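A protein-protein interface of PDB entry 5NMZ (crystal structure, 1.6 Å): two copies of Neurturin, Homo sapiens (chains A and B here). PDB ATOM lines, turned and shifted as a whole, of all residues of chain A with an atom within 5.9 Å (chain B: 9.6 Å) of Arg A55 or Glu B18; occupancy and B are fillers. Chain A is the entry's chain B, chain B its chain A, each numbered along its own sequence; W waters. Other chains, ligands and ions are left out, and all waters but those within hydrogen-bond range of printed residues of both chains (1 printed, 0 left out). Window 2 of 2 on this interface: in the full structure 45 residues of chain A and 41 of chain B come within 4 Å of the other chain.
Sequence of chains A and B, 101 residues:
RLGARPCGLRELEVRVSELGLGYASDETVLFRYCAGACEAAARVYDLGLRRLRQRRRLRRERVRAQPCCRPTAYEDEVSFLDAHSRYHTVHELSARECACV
The backbone NH (N) of Phe B31 lies within hydrogen-bond range of the backbone carbonyl oxygen (O) of Leu B12, at 2.8 Å.
The backbone NH (N) of Val B29 lies within hydrogen-bond range of the backbone carbonyl oxygen (O) of Val B14 (2.9 Å).
The guanidinium group (NE) of Arg B15 lies within salt-bridge range of the side-chain carboxylate (OE1) of Glu B18 (3.8 Å).
NE2 of Gln A54 lies within hydrogen-bond range of O of Arg A51 (2.8 Å).
O of Leu A52 sits at hydrogen-bond distance from N of Arg A57, 3.2 Å away.
Water W1 lies within hydrogen-bond range of O of Glu B13 (2.9 Å) and NH1 of Arg A57 (3.0 Å).
No position is printed for both chains.
Of the 11 pairs that touch across the chains among the printed residues, none has its exchanged pair printed and touching as well.
Of the 9 printed residues of chain A, 5 touch a printed residue of chain B.
Printed residues of chain A that touch a printed residue of chain B: Gly A48, Arg A51, Leu A52, Arg A55 and Arg A57.
Hydrophobic or aromatic side chains of chain A within 4 Å of the printed part of chain B: Leu A52.
Among the printed residues, 11 pairs touch across the chains.
Among the printed residues, Asp or Glu carboxylates within 4 Å of a Lys or Arg side-chain nitrogen of the other chain: Arg A55 with Glu B18 and Arg A57 with Glu B18.
The guanidinium group of Arg A57 is in hydrogen-bond range of the backbone carbonyl oxygen of Glu B13 (2.9 Å).
The side-chain carboxylate (OE2) of Glu B18 is in salt-bridge range of the guanidinium group (NH2) of Arg A55 (3.0 Å).
OE2 of Glu B18 lies within salt-bridge range of NE of Arg A57 (2.9 Å).
Among the printed residues, pairs that only touch across the chains: Arg A57 with Leu B12, Arg A57 with Val B14, Gly A48 with Leu B19, Leu A52 with Phe B31, Arg A51 with Glu B18, Arg A51 with Leu B19, Leu A52 with Val B14 and Leu A52 with Leu B19.
Glu B18 touches just these residues of chain A: Arg A51 (3.6 Å), Arg A55 (3.0 Å) and Arg A57 (2.9 Å).
Gln A54 touches none of the printed residues of chain B.
Of the printed residues of chain B, Leu A52 touches Val B14, Leu B19 and Phe B31.
Of the printed residues of chain A, Val B14 touches Leu A52 (3.8 Å) and Arg A57 (3.3 Å).
Asp B26 touches none of the printed residues of chain A.
Tyr B23 touches none of the printed residues of chain A.
The nearest residue of chain B that does not touch Arg A55 is Arg B15 (4.5 Å).
The nearest printed residue of chain B that does not touch Arg A57 is Arg B15 (5.1 Å).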
ATOM      1  N   GLY A  48     -14.003   6.193  16.869  1.00  0.00           N
ATOM      2  CA  GLY A  48     -14.173   7.070  15.728  1.00  0.00           C
ATOM      3  C   GLY A  48     -15.279   6.608  14.795  1.00  0.00           C
ATOM      4  O   GLY A  48     -16.123   7.404  14.406  1.00  0.00           O
ATOM      5  N   ARG A  50     -17.921   4.684  15.512  1.00  0.00           N
ATOM      6  CA  ARG A  50     -19.218   4.873  16.194  1.00  0.00           C
ATOM      7  C   ARG A  50     -19.658   6.345  16.163  1.00  0.00           C
ATOM      8  O   ARG A  50     -20.844   6.618  15.936  1.00  0.00           O
ATOM      9  CB  ARG A  50     -19.131   4.401  17.657  1.00  0.00           C
ATOM     10  CG  ARG A  50     -19.603   2.983  17.874  1.00  0.00           C
ATOM     11  CD  ARG A  50     -19.785   2.667  19.344  1.00  0.00           C
ATOM     12  NE  ARG A  50     -18.535   2.729  20.110  1.00  0.00           N
ATOM     13  CZ  ARG A  50     -17.807   1.670  20.460  1.00  0.00           C
ATOM     14  NH1 ARG A  50     -16.702   1.827  21.175  1.00  0.00           N
ATOM     15  NH2 ARG A  50     -18.189   0.447  20.112  1.00  0.00           N
ATOM     16  N   ARG A  51     -18.709   7.282  16.333  1.00  0.00           N
ATOM     17  CA  ARG A  51     -18.933   8.743  16.298  1.00  0.00           C
ATOM     18  C   ARG A  51     -19.372   9.207  14.897  1.00  0.00           C
ATOM     19  O   ARG A  51     -20.238  10.075  14.793  1.00  0.00           O
ATOM     20  CB  ARG A  51     -17.690   9.505  16.797  1.00  0.00           C
ATOM     21  CG  ARG A  51     -17.417   9.334  18.302  1.00  0.00           C
ATOM     22  CD  ARG A  51     -18.378  10.119  19.218  1.00  0.00           C
ATOM     23  NE  ARG A  51     -18.104   9.802  20.621  1.00  0.00           N
ATOM     24  CZ  ARG A  51     -18.733   8.873  21.328  1.00  0.00           C
ATOM     25  NH1 ARG A  51     -19.721   8.170  20.784  1.00  0.00           N
ATOM     26  NH2 ARG A  51     -18.374   8.634  22.590  1.00  0.00           N
ATOM     27  N   LEU A  52     -18.867   8.561  13.841  1.00  0.00           N
ATOM     28  CA  LEU A  52     -19.218   8.829  12.430  1.00  0.00           C
ATOM     29  C   LEU A  52     -20.513   8.155  11.976  1.00  0.00           C
ATOM     30  O   LEU A  52     -21.247   8.735  11.173  1.00  0.00           O
ATOM     31  CB  LEU A  52     -18.081   8.418  11.476  1.00  0.00           C
ATOM     32  CG  LEU A  52     -16.795   9.231  11.574  1.00  0.00           C
ATOM     33  CD1 LEU A  52     -15.684   8.567  10.768  1.00  0.00           C
ATOM     34  CD2 LEU A  52     -16.990  10.651  11.039  1.00  0.00           C
ATOM     35  N   ARG A  53     -20.796   6.916  12.453  1.00  0.00           N
ATOM     36  CA  ARG A  53     -22.024   6.241  12.039  1.00  0.00           C
ATOM     37  C   ARG A  53     -23.230   7.049  12.542  1.00  0.00           C
ATOM     38  O   ARG A  53     -24.157   7.311  11.776  1.00  0.00           O
ATOM     39  CB  ARG A  53     -22.040   4.777  12.540  1.00  0.00           C
ATOM     40  CG  ARG A  53     -23.383   4.096  12.330  1.00  0.00           C
ATOM     41  CD  ARG A  53     -23.362   2.627  12.665  1.00  0.00           C
ATOM     42  NE  ARG A  53     -23.277   2.392  14.106  1.00  0.00           N
ATOM     43  CZ  ARG A  53     -22.937   1.228  14.646  1.00  0.00           C
ATOM     44  NH1 ARG A  53     -22.653   0.187  13.868  1.00  0.00           N
ATOM     45  NH2 ARG A  53     -22.904   1.085  15.969  1.00  0.00           N
ATOM     46  N   GLN A  54     -23.151   7.517  13.791  1.00  0.00           N
ATOM     47  CA  GLN A  54     -24.185   8.268  14.500  1.00  0.00           C
ATOM     48  C   GLN A  54     -24.541   9.554  13.797  1.00  0.00           C
ATOM     49  O   GLN A  54     -25.684  10.005  13.906  1.00  0.00           O
ATOM     50  CB  GLN A  54     -23.769   8.474  15.989  1.00  0.00           C
ATOM     51  CG  GLN A  54     -23.779   9.919  16.546  1.00  0.00           C
ATOM     52  CD  GLN A  54     -22.496  10.326  17.254  1.00  0.00           C
ATOM     53  OE1 GLN A  54     -22.118   9.777  18.304  1.00  0.00           O
ATOM     54  NE2 GLN A  54     -21.826  11.349  16.730  1.00  0.00           N
ATOM     55  N   ARG A  55     -23.587  10.139  13.082  1.00  0.00           N
ATOM     56  CA  ARG A  55     -23.793  11.375  12.361  1.00  0.00           C
ATOM     57  C   ARG A  55     -24.134  11.140  10.890  1.00  0.00           C
ATOM     58  O   ARG A  55     -24.119  12.101  10.109  1.00  0.00           O
ATOM     59  CB  ARG A  55     -22.574  12.293  12.547  1.00  0.00           C
ATOM     60  CG  ARG A  55     -22.631  13.109  13.844  1.00  0.00           C
ATOM     61  CD  ARG A  55     -21.336  13.835  14.186  1.00  0.00           C
ATOM     62  NE  ARG A  55     -21.010  14.896  13.226  1.00  0.00           N
ATOM     63  CZ  ARG A  55     -20.012  14.830  12.347  1.00  0.00           C
ATOM     64  NH1 ARG A  55     -19.249  13.745  12.274  1.00  0.00           N
ATOM     65  NH2 ARG A  55     -19.787  15.836  11.514  1.00  0.00           N
ATOM     66  N   ARG A  56     -24.471   9.868  10.495  1.00  0.00           N
ATOM     67  CA  ARG A  56     -24.840   9.487   9.122  1.00  0.00           C
ATOM     68  C   ARG A  56     -23.762   9.832   8.045  1.00  0.00           C
ATOM     69  O   ARG A  56     -24.089  10.103   6.882  1.00  0.00           O
ATOM     70  CB  ARG A  56     -26.229  10.071   8.729  1.00  0.00           C
ATOM     71  CG  ARG A  56     -27.414   9.290   9.310  1.00  0.00           C
ATOM     72  CD  ARG A  56     -28.755   9.986   9.038  1.00  0.00           C
ATOM     73  NE  ARG A  56     -29.053  10.140   7.607  1.00  0.00           N
ATOM     74  CZ  ARG A  56     -29.679  11.189   7.071  1.00  0.00           C
ATOM     75  NH1 ARG A  56     -30.088  12.193   7.839  1.00  0.00           N
ATOM     76  NH2 ARG A  56     -29.898  11.242   5.763  1.00  0.00           N
ATOM     77  N   ARG A  57     -22.482   9.781   8.433  1.00  0.00           N
ATOM     78  CA  ARG A  57     -21.339  10.032   7.557  1.00  0.00           C
ATOM     79  C   ARG A  57     -20.851   8.769   6.768  1.00  0.00           C
ATOM     80  O   ARG A  57     -19.871   8.871   6.025  1.00  0.00           O
ATOM     81  CB  ARG A  57     -20.177  10.627   8.380  1.00  0.00           C
ATOM     82  CG  ARG A  57     -20.506  11.993   8.992  1.00  0.00           C
ATOM     83  CD  ARG A  57     -20.082  13.095   8.056  1.00  0.00           C
ATOM     84  NE  ARG A  57     -18.669  13.411   8.250  1.00  0.00           N
ATOM     85  CZ  ARG A  57     -17.821  13.638   7.265  1.00  0.00           C
ATOM     86  NH1 ARG A  57     -18.230  13.586   6.002  1.00  0.00           N
ATOM     87  NH2 ARG A  57     -16.557  13.921   7.528  1.00  0.00           N
ATOM     88  N   LEU B  12     -12.843   8.206   4.030  1.00  0.00           N
ATOM     89  CA  LEU B  12     -13.660   9.392   4.211  1.00  0.00           C
ATOM     90  C   LEU B  12     -12.809  10.524   4.810  1.00  0.00           C
ATOM     91  O   LEU B  12     -12.073  10.304   5.757  1.00  0.00           O
ATOM     92  CB  LEU B  12     -14.829   9.053   5.181  1.00  0.00           C
ATOM     93  CG  LEU B  12     -15.878  10.119   5.456  1.00  0.00           C
ATOM     94  CD1 LEU B  12     -16.773  10.311   4.254  1.00  0.00           C
ATOM     95  CD2 LEU B  12     -16.742   9.720   6.668  1.00  0.00           C
ATOM     96  N   GLU B  13     -12.897  11.751   4.233  1.00  0.00           N
ATOM     97  CA  GLU B  13     -12.159  12.881   4.806  1.00  0.00           C
ATOM     98  C   GLU B  13     -12.921  13.362   6.033  1.00  0.00           C
ATOM     99  O   GLU B  13     -14.128  13.606   5.948  1.00  0.00           O
ATOM    100  CB  GLU B  13     -12.063  14.062   3.818  1.00  0.00           C
ATOM    101  CG  GLU B  13     -11.287  13.739   2.559  1.00  0.00           C
ATOM    102  CD  GLU B  13     -11.101  14.923   1.628  1.00  0.00           C
ATOM    103  OE1 GLU B  13     -12.088  15.644   1.347  1.00  0.00           O
ATOM    104  OE2 GLU B  13      -9.954  15.123   1.169  1.00  0.00           O
ATOM    105  N   VAL B  14     -12.238  13.466   7.186  1.00  0.00           N
ATOM    106  CA  VAL B  14     -12.853  13.896   8.436  1.00  0.00           C
ATOM    107  C   VAL B  14     -11.932  14.807   9.223  1.00  0.00           C
ATOM    108  O   VAL B  14     -10.724  14.623   9.205  1.00  0.00           O
ATOM    109  CB  VAL B  14     -13.289  12.683   9.340  1.00  0.00           C
ATOM    110  CG1 VAL B  14     -14.294  11.776   8.651  1.00  0.00           C
ATOM    111  CG2 VAL B  14     -12.092  11.872   9.830  1.00  0.00           C
ATOM    112  N   ARG B  15     -12.507  15.730   9.995  1.00  0.00           N
ATOM    113  CA  ARG B  15     -11.726  16.560  10.889  1.00  0.00           C
ATOM    114  C   ARG B  15     -11.479  15.696  12.116  1.00  0.00           C
ATOM    115  O   ARG B  15     -12.373  14.961  12.515  1.00  0.00           O
ATOM    116  CB  ARG B  15     -12.513  17.816  11.306  1.00  0.00           C
ATOM    117  CG  ARG B  15     -12.580  18.869  10.182  1.00  0.00           C
ATOM    118  CD  ARG B  15     -13.476  20.044  10.548  1.00  0.00           C
ATOM    119  NE  ARG B  15     -14.889  19.665  10.528  1.00  0.00           N
ATOM    120  CZ  ARG B  15     -15.649  19.621  11.612  1.00  0.00           C
ATOM    121  NH1 ARG B  15     -15.148  19.953  12.795  1.00  0.00           N
ATOM    122  NH2 ARG B  15     -16.920  19.255  11.525  1.00  0.00           N
ATOM    123  N   VAL B  16     -10.272  15.776  12.729  1.00  0.00           N
ATOM    124  CA  VAL B  16      -9.950  14.939  13.889  1.00  0.00           C
ATOM    125  C   VAL B  16     -11.003  15.119  15.017  1.00  0.00           C
ATOM    126  O   VAL B  16     -11.408  14.101  15.579  1.00  0.00           O
ATOM    127  CB  VAL B  16      -8.483  15.089  14.366  1.00  0.00           C
ATOM    128  CG1 VAL B  16      -8.214  14.339  15.677  1.00  0.00           C
ATOM    129  CG2 VAL B  16      -7.526  14.608  13.280  1.00  0.00           C
ATOM    130  N   SER B  17     -11.550  16.349  15.243  1.00  0.00           N
ATOM    131  CA  SER B  17     -12.647  16.594  16.201  1.00  0.00           C
ATOM    132  C   SER B  17     -13.829  15.625  16.008  1.00  0.00           C
ATOM    133  O   SER B  17     -14.404  15.149  17.000  1.00  0.00           O
ATOM    134  CB  SER B  17     -13.179  18.016  16.086  1.00  0.00           C
ATOM    135  OG  SER B  17     -12.224  18.951  16.539  1.00  0.00           O
ATOM    136  N   GLU B  18     -14.157  15.265  14.740  1.00  0.00           N
ATOM    137  CA  GLU B  18     -15.284  14.387  14.410  1.00  0.00           C
ATOM    138  C   GLU B  18     -15.165  12.978  14.965  1.00  0.00           C
ATOM    139  O   GLU B  18     -16.176  12.312  15.152  1.00  0.00           O
ATOM    140  CB  GLU B  18     -15.534  14.318  12.887  1.00  0.00           C
ATOM    141  CG  GLU B  18     -16.049  15.610  12.264  1.00  0.00           C
ATOM    142  CD  GLU B  18     -16.216  15.501  10.761  1.00  0.00           C
ATOM    143  OE1 GLU B  18     -15.272  15.883  10.037  1.00  0.00           O
ATOM    144  OE2 GLU B  18     -17.227  14.911  10.309  1.00  0.00           O
ATOM    145  N   LEU B  19     -13.939  12.513  15.170  1.00  0.00           N
ATOM    146  CA  LEU B  19     -13.624  11.178  15.692  1.00  0.00           C
ATOM    147  C   LEU B  19     -13.848  11.055  17.223  1.00  0.00           C
ATOM    148  O   LEU B  19     -13.890   9.951  17.720  1.00  0.00           O
ATOM    149  CB  LEU B  19     -12.198  10.811  15.287  1.00  0.00           C
ATOM    150  CG  LEU B  19     -11.963  10.735  13.743  1.00  0.00           C
ATOM    151  CD1 LEU B  19     -10.475  10.597  13.411  1.00  0.00           C
ATOM    152  CD2 LEU B  19     -12.702   9.602  13.106  1.00  0.00           C
ATOM    153  N   GLY B  20     -13.986  12.189  17.917  1.00  0.00           N
ATOM    154  CA  GLY B  20     -14.233  12.256  19.356  1.00  0.00           C
ATOM    155  C   GLY B  20     -13.189  11.616  20.234  1.00  0.00           C
ATOM    156  O   GLY B  20     -13.524  10.960  21.234  1.00  0.00           O
ATOM    157  N   LEU B  21     -11.903  11.838  19.895  1.00  0.00           N
ATOM    158  CA  LEU B  21     -10.769  11.231  20.617  1.00  0.00           C
ATOM    159  C   LEU B  21     -10.450  11.891  21.951  1.00  0.00           C
ATOM    160  O   LEU B  21      -9.615  11.385  22.713  1.00  0.00           O
ATOM    161  CB  LEU B  21      -9.517  11.330  19.729  1.00  0.00           C
ATOM    162  CG  LEU B  21      -9.667  10.734  18.295  1.00  0.00           C
ATOM    163  CD1 LEU B  21      -8.380  10.816  17.568  1.00  0.00           C
ATOM    164  CD2 LEU B  21     -10.142   9.290  18.316  1.00  0.00           C
ATOM    165  N   GLY B  22     -11.054  13.027  22.197  1.00  0.00           N
ATOM    166  CA  GLY B  22     -10.802  13.763  23.419  1.00  0.00           C
ATOM    167  C   GLY B  22     -10.162  15.096  23.192  1.00  0.00           C
ATOM    168  O   GLY B  22     -10.005  15.860  24.143  1.00  0.00           O
ATOM    169  N   TYR B  23      -9.808  15.403  21.932  1.00  0.00           N
ATOM    170  CA  TYR B  23      -9.104  16.647  21.616  1.00  0.00           C
ATOM    171  C   TYR B  23      -9.750  17.292  20.438  1.00  0.00           C
ATOM    172  O   TYR B  23     -10.173  16.608  19.511  1.00  0.00           O
ATOM    173  CB  TYR B  23      -7.616  16.369  21.295  1.00  0.00           C
ATOM    174  CG  TYR B  23      -6.966  15.449  22.301  1.00  0.00           C
ATOM    175  CD1 TYR B  23      -6.574  15.918  23.553  1.00  0.00           C
ATOM    176  CD2 TYR B  23      -6.792  14.096  22.029  1.00  0.00           C
ATOM    177  CE1 TYR B  23      -6.068  15.054  24.522  1.00  0.00           C
ATOM    178  CE2 TYR B  23      -6.270  13.225  22.985  1.00  0.00           C
ATOM    179  CZ  TYR B  23      -5.905  13.712  24.230  1.00  0.00           C
ATOM    180  OH  TYR B  23      -5.363  12.874  25.172  1.00  0.00           O
ATOM    181  N   ALA B  24      -9.860  18.596  20.482  1.00  0.00           N
ATOM    182  CA  ALA B  24     -10.427  19.371  19.378  1.00  0.00           C
ATOM    183  C   ALA B  24      -9.285  19.641  18.402  1.00  0.00           C
ATOM    184  O   ALA B  24      -8.200  20.035  18.813  1.00  0.00           O
ATOM    185  CB  ALA B  24     -11.013  20.689  19.896  1.00  0.00           C
ATOM    186  N   SER B  25      -9.498  19.352  17.119  1.00  0.00           N
ATOM    187  CA  SER B  25      -8.525  19.623  16.061  1.00  0.00           C
ATOM    188  C   SER B  25      -9.251  19.734  14.745  1.00  0.00           C
ATOM    189  O   SER B  25     -10.091  18.881  14.419  1.00  0.00           O
ATOM    190  CB  SER B  25      -7.442  18.554  15.997  1.00  0.00           C
ATOM    191  OG  SER B  25      -6.608  18.784  14.872  1.00  0.00           O
ATOM    192  N   ASP B  26      -8.944  20.791  13.996  1.00  0.00           N
ATOM    193  CA  ASP B  26      -9.576  20.998  12.691  1.00  0.00           C
ATOM    194  C   ASP B  26      -8.766  20.369  11.550  1.00  0.00           C
ATOM    195  O   ASP B  26      -9.152  20.496  10.390  1.00  0.00           O
ATOM    196  CB  ASP B  26      -9.897  22.476  12.453  1.00  0.00           C
ATOM    197  CG  ASP B  26     -10.982  23.009  13.369  1.00  0.00           C
ATOM    198  OD1 ASP B  26     -12.138  22.495  13.300  1.00  0.00           O
ATOM    199  OD2 ASP B  26     -10.689  23.950  14.147  1.00  0.00           O
ATOM    200  N   GLU B  27      -7.675  19.644  11.887  1.00  0.00           N
ATOM    201  CA  GLU B  27      -6.828  18.924  10.935  1.00  0.00           C
ATOM    202  C   GLU B  27      -7.686  17.850  10.286  1.00  0.00           C
ATOM    203  O   GLU B  27      -8.406  17.132  10.989  1.00  0.00           O
ATOM    204  CB  GLU B  27      -5.656  18.251  11.651  1.00  0.00           C
ATOM    205  CG  GLU B  27      -4.442  17.974  10.784  1.00  0.00           C
ATOM    206  CD  GLU B  27      -3.230  17.514  11.572  1.00  0.00           C
ATOM    207  OE1 GLU B  27      -2.831  18.216  12.525  1.00  0.00           O
ATOM    208  OE2 GLU B  27      -2.665  16.452  11.232  1.00  0.00           O
ATOM    209  N   THR B  28      -7.627  17.772   8.955  1.00  0.00           N
ATOM    210  CA  THR B  28      -8.393  16.800   8.182  1.00  0.00           C
ATOM    211  C   THR B  28      -7.557  15.584   7.868  1.00  0.00           C
ATOM    212  O   THR B  28      -6.468  15.701   7.312  1.00  0.00           O
ATOM    213  CB  THR B  28      -8.931  17.457   6.904  1.00  0.00           C
ATOM    214  OG1 THR B  28      -7.859  18.220   6.338  1.00  0.00           O
ATOM    215  CG2 THR B  28     -10.106  18.359   7.168  1.00  0.00           C
ATOM    216  N   VAL B  29      -8.059  14.389   8.207  1.00  0.00           N
ATOM    217  CA  VAL B  29      -7.373  13.160   7.881  1.00  0.00           C
ATOM    218  C   VAL B  29      -8.243  12.335   6.949  1.00  0.00           C
ATOM    219  O   VAL B  29      -9.464  12.548   6.889  1.00  0.00           O
ATOM    220  CB  VAL B  29      -6.921  12.368   9.135  1.00  0.00           C
ATOM    221  CG1 VAL B  29      -5.921  13.175   9.967  1.00  0.00           C
ATOM    222  CG2 VAL B  29      -8.111  11.924   9.977  1.00  0.00           C
ATOM    223  N   PHE B  31      -9.789   9.143   6.886  1.00  0.00           N
ATOM    224  CA  PHE B  31     -10.116   8.027   7.780  1.00  0.00           C
ATOM    225  C   PHE B  31     -10.491   6.831   6.947  1.00  0.00           C
ATOM    226  O   PHE B  31     -11.297   6.959   6.043  1.00  0.00           O
ATOM    227  CB  PHE B  31     -11.226   8.411   8.704  1.00  0.00           C
ATOM    228  CG  PHE B  31     -11.692   7.324   9.648  1.00  0.00           C
ATOM    229  CD1 PHE B  31     -10.897   6.930  10.732  1.00  0.00           C
ATOM    230  CD2 PHE B  31     -12.948   6.744   9.495  1.00  0.00           C
ATOM    231  CE1 PHE B  31     -11.327   5.926  11.609  1.00  0.00           C
ATOM    232  CE2 PHE B  31     -13.388   5.755  10.390  1.00  0.00           C
ATOM    233  CZ  PHE B  31     -12.585   5.391  11.454  1.00  0.00           C
ATOM    234  N   PHE B  80      -1.399  14.344  14.961  1.00  0.00           N
ATOM    235  CA  PHE B  80      -2.067  15.609  14.712  1.00  0.00           C
ATOM    236  C   PHE B  80      -1.768  16.575  15.856  1.00  0.00           C
ATOM    237  O   PHE B  80      -1.392  16.152  16.947  1.00  0.00           O
ATOM    238  CB  PHE B  80      -3.594  15.421  14.505  1.00  0.00           C
ATOM    239  CG  PHE B  80      -4.260  14.774  15.695  1.00  0.00           C
ATOM    240  CD1 PHE B  80      -4.700  15.546  16.773  1.00  0.00           C
ATOM    241  CD2 PHE B  80      -4.434  13.395  15.750  1.00  0.00           C
ATOM    242  CE1 PHE B  80      -5.293  14.945  17.888  1.00  0.00           C
ATOM    243  CE2 PHE B  80      -5.030  12.800  16.855  1.00  0.00           C
ATOM    244  CZ  PHE B  80      -5.440  13.575  17.925  1.00  0.00           C
ATOM    245  N   LEU B  93      -5.678   3.896  14.261  1.00  0.00           N
ATOM    246  CA  LEU B  93      -6.923   4.651  14.175  1.00  0.00           C
ATOM    247  C   LEU B  93      -7.691   4.211  12.958  1.00  0.00           C
ATOM    248  O   LEU B  93      -8.904   4.049  13.047  1.00  0.00           O
ATOM    249  CB  LEU B  93      -6.657   6.157  14.100  1.00  0.00           C
ATOM    250  CG  LEU B  93      -7.895   7.025  13.810  1.00  0.00           C
ATOM    251  CD1 LEU B  93      -8.882   6.963  14.963  1.00  0.00           C
ATOM    252  CD2 LEU B  93      -7.500   8.459  13.485  1.00  0.00           C
HETATM  253  O   HOH W   1     -16.109  14.002   3.911  1.00  0.00           O
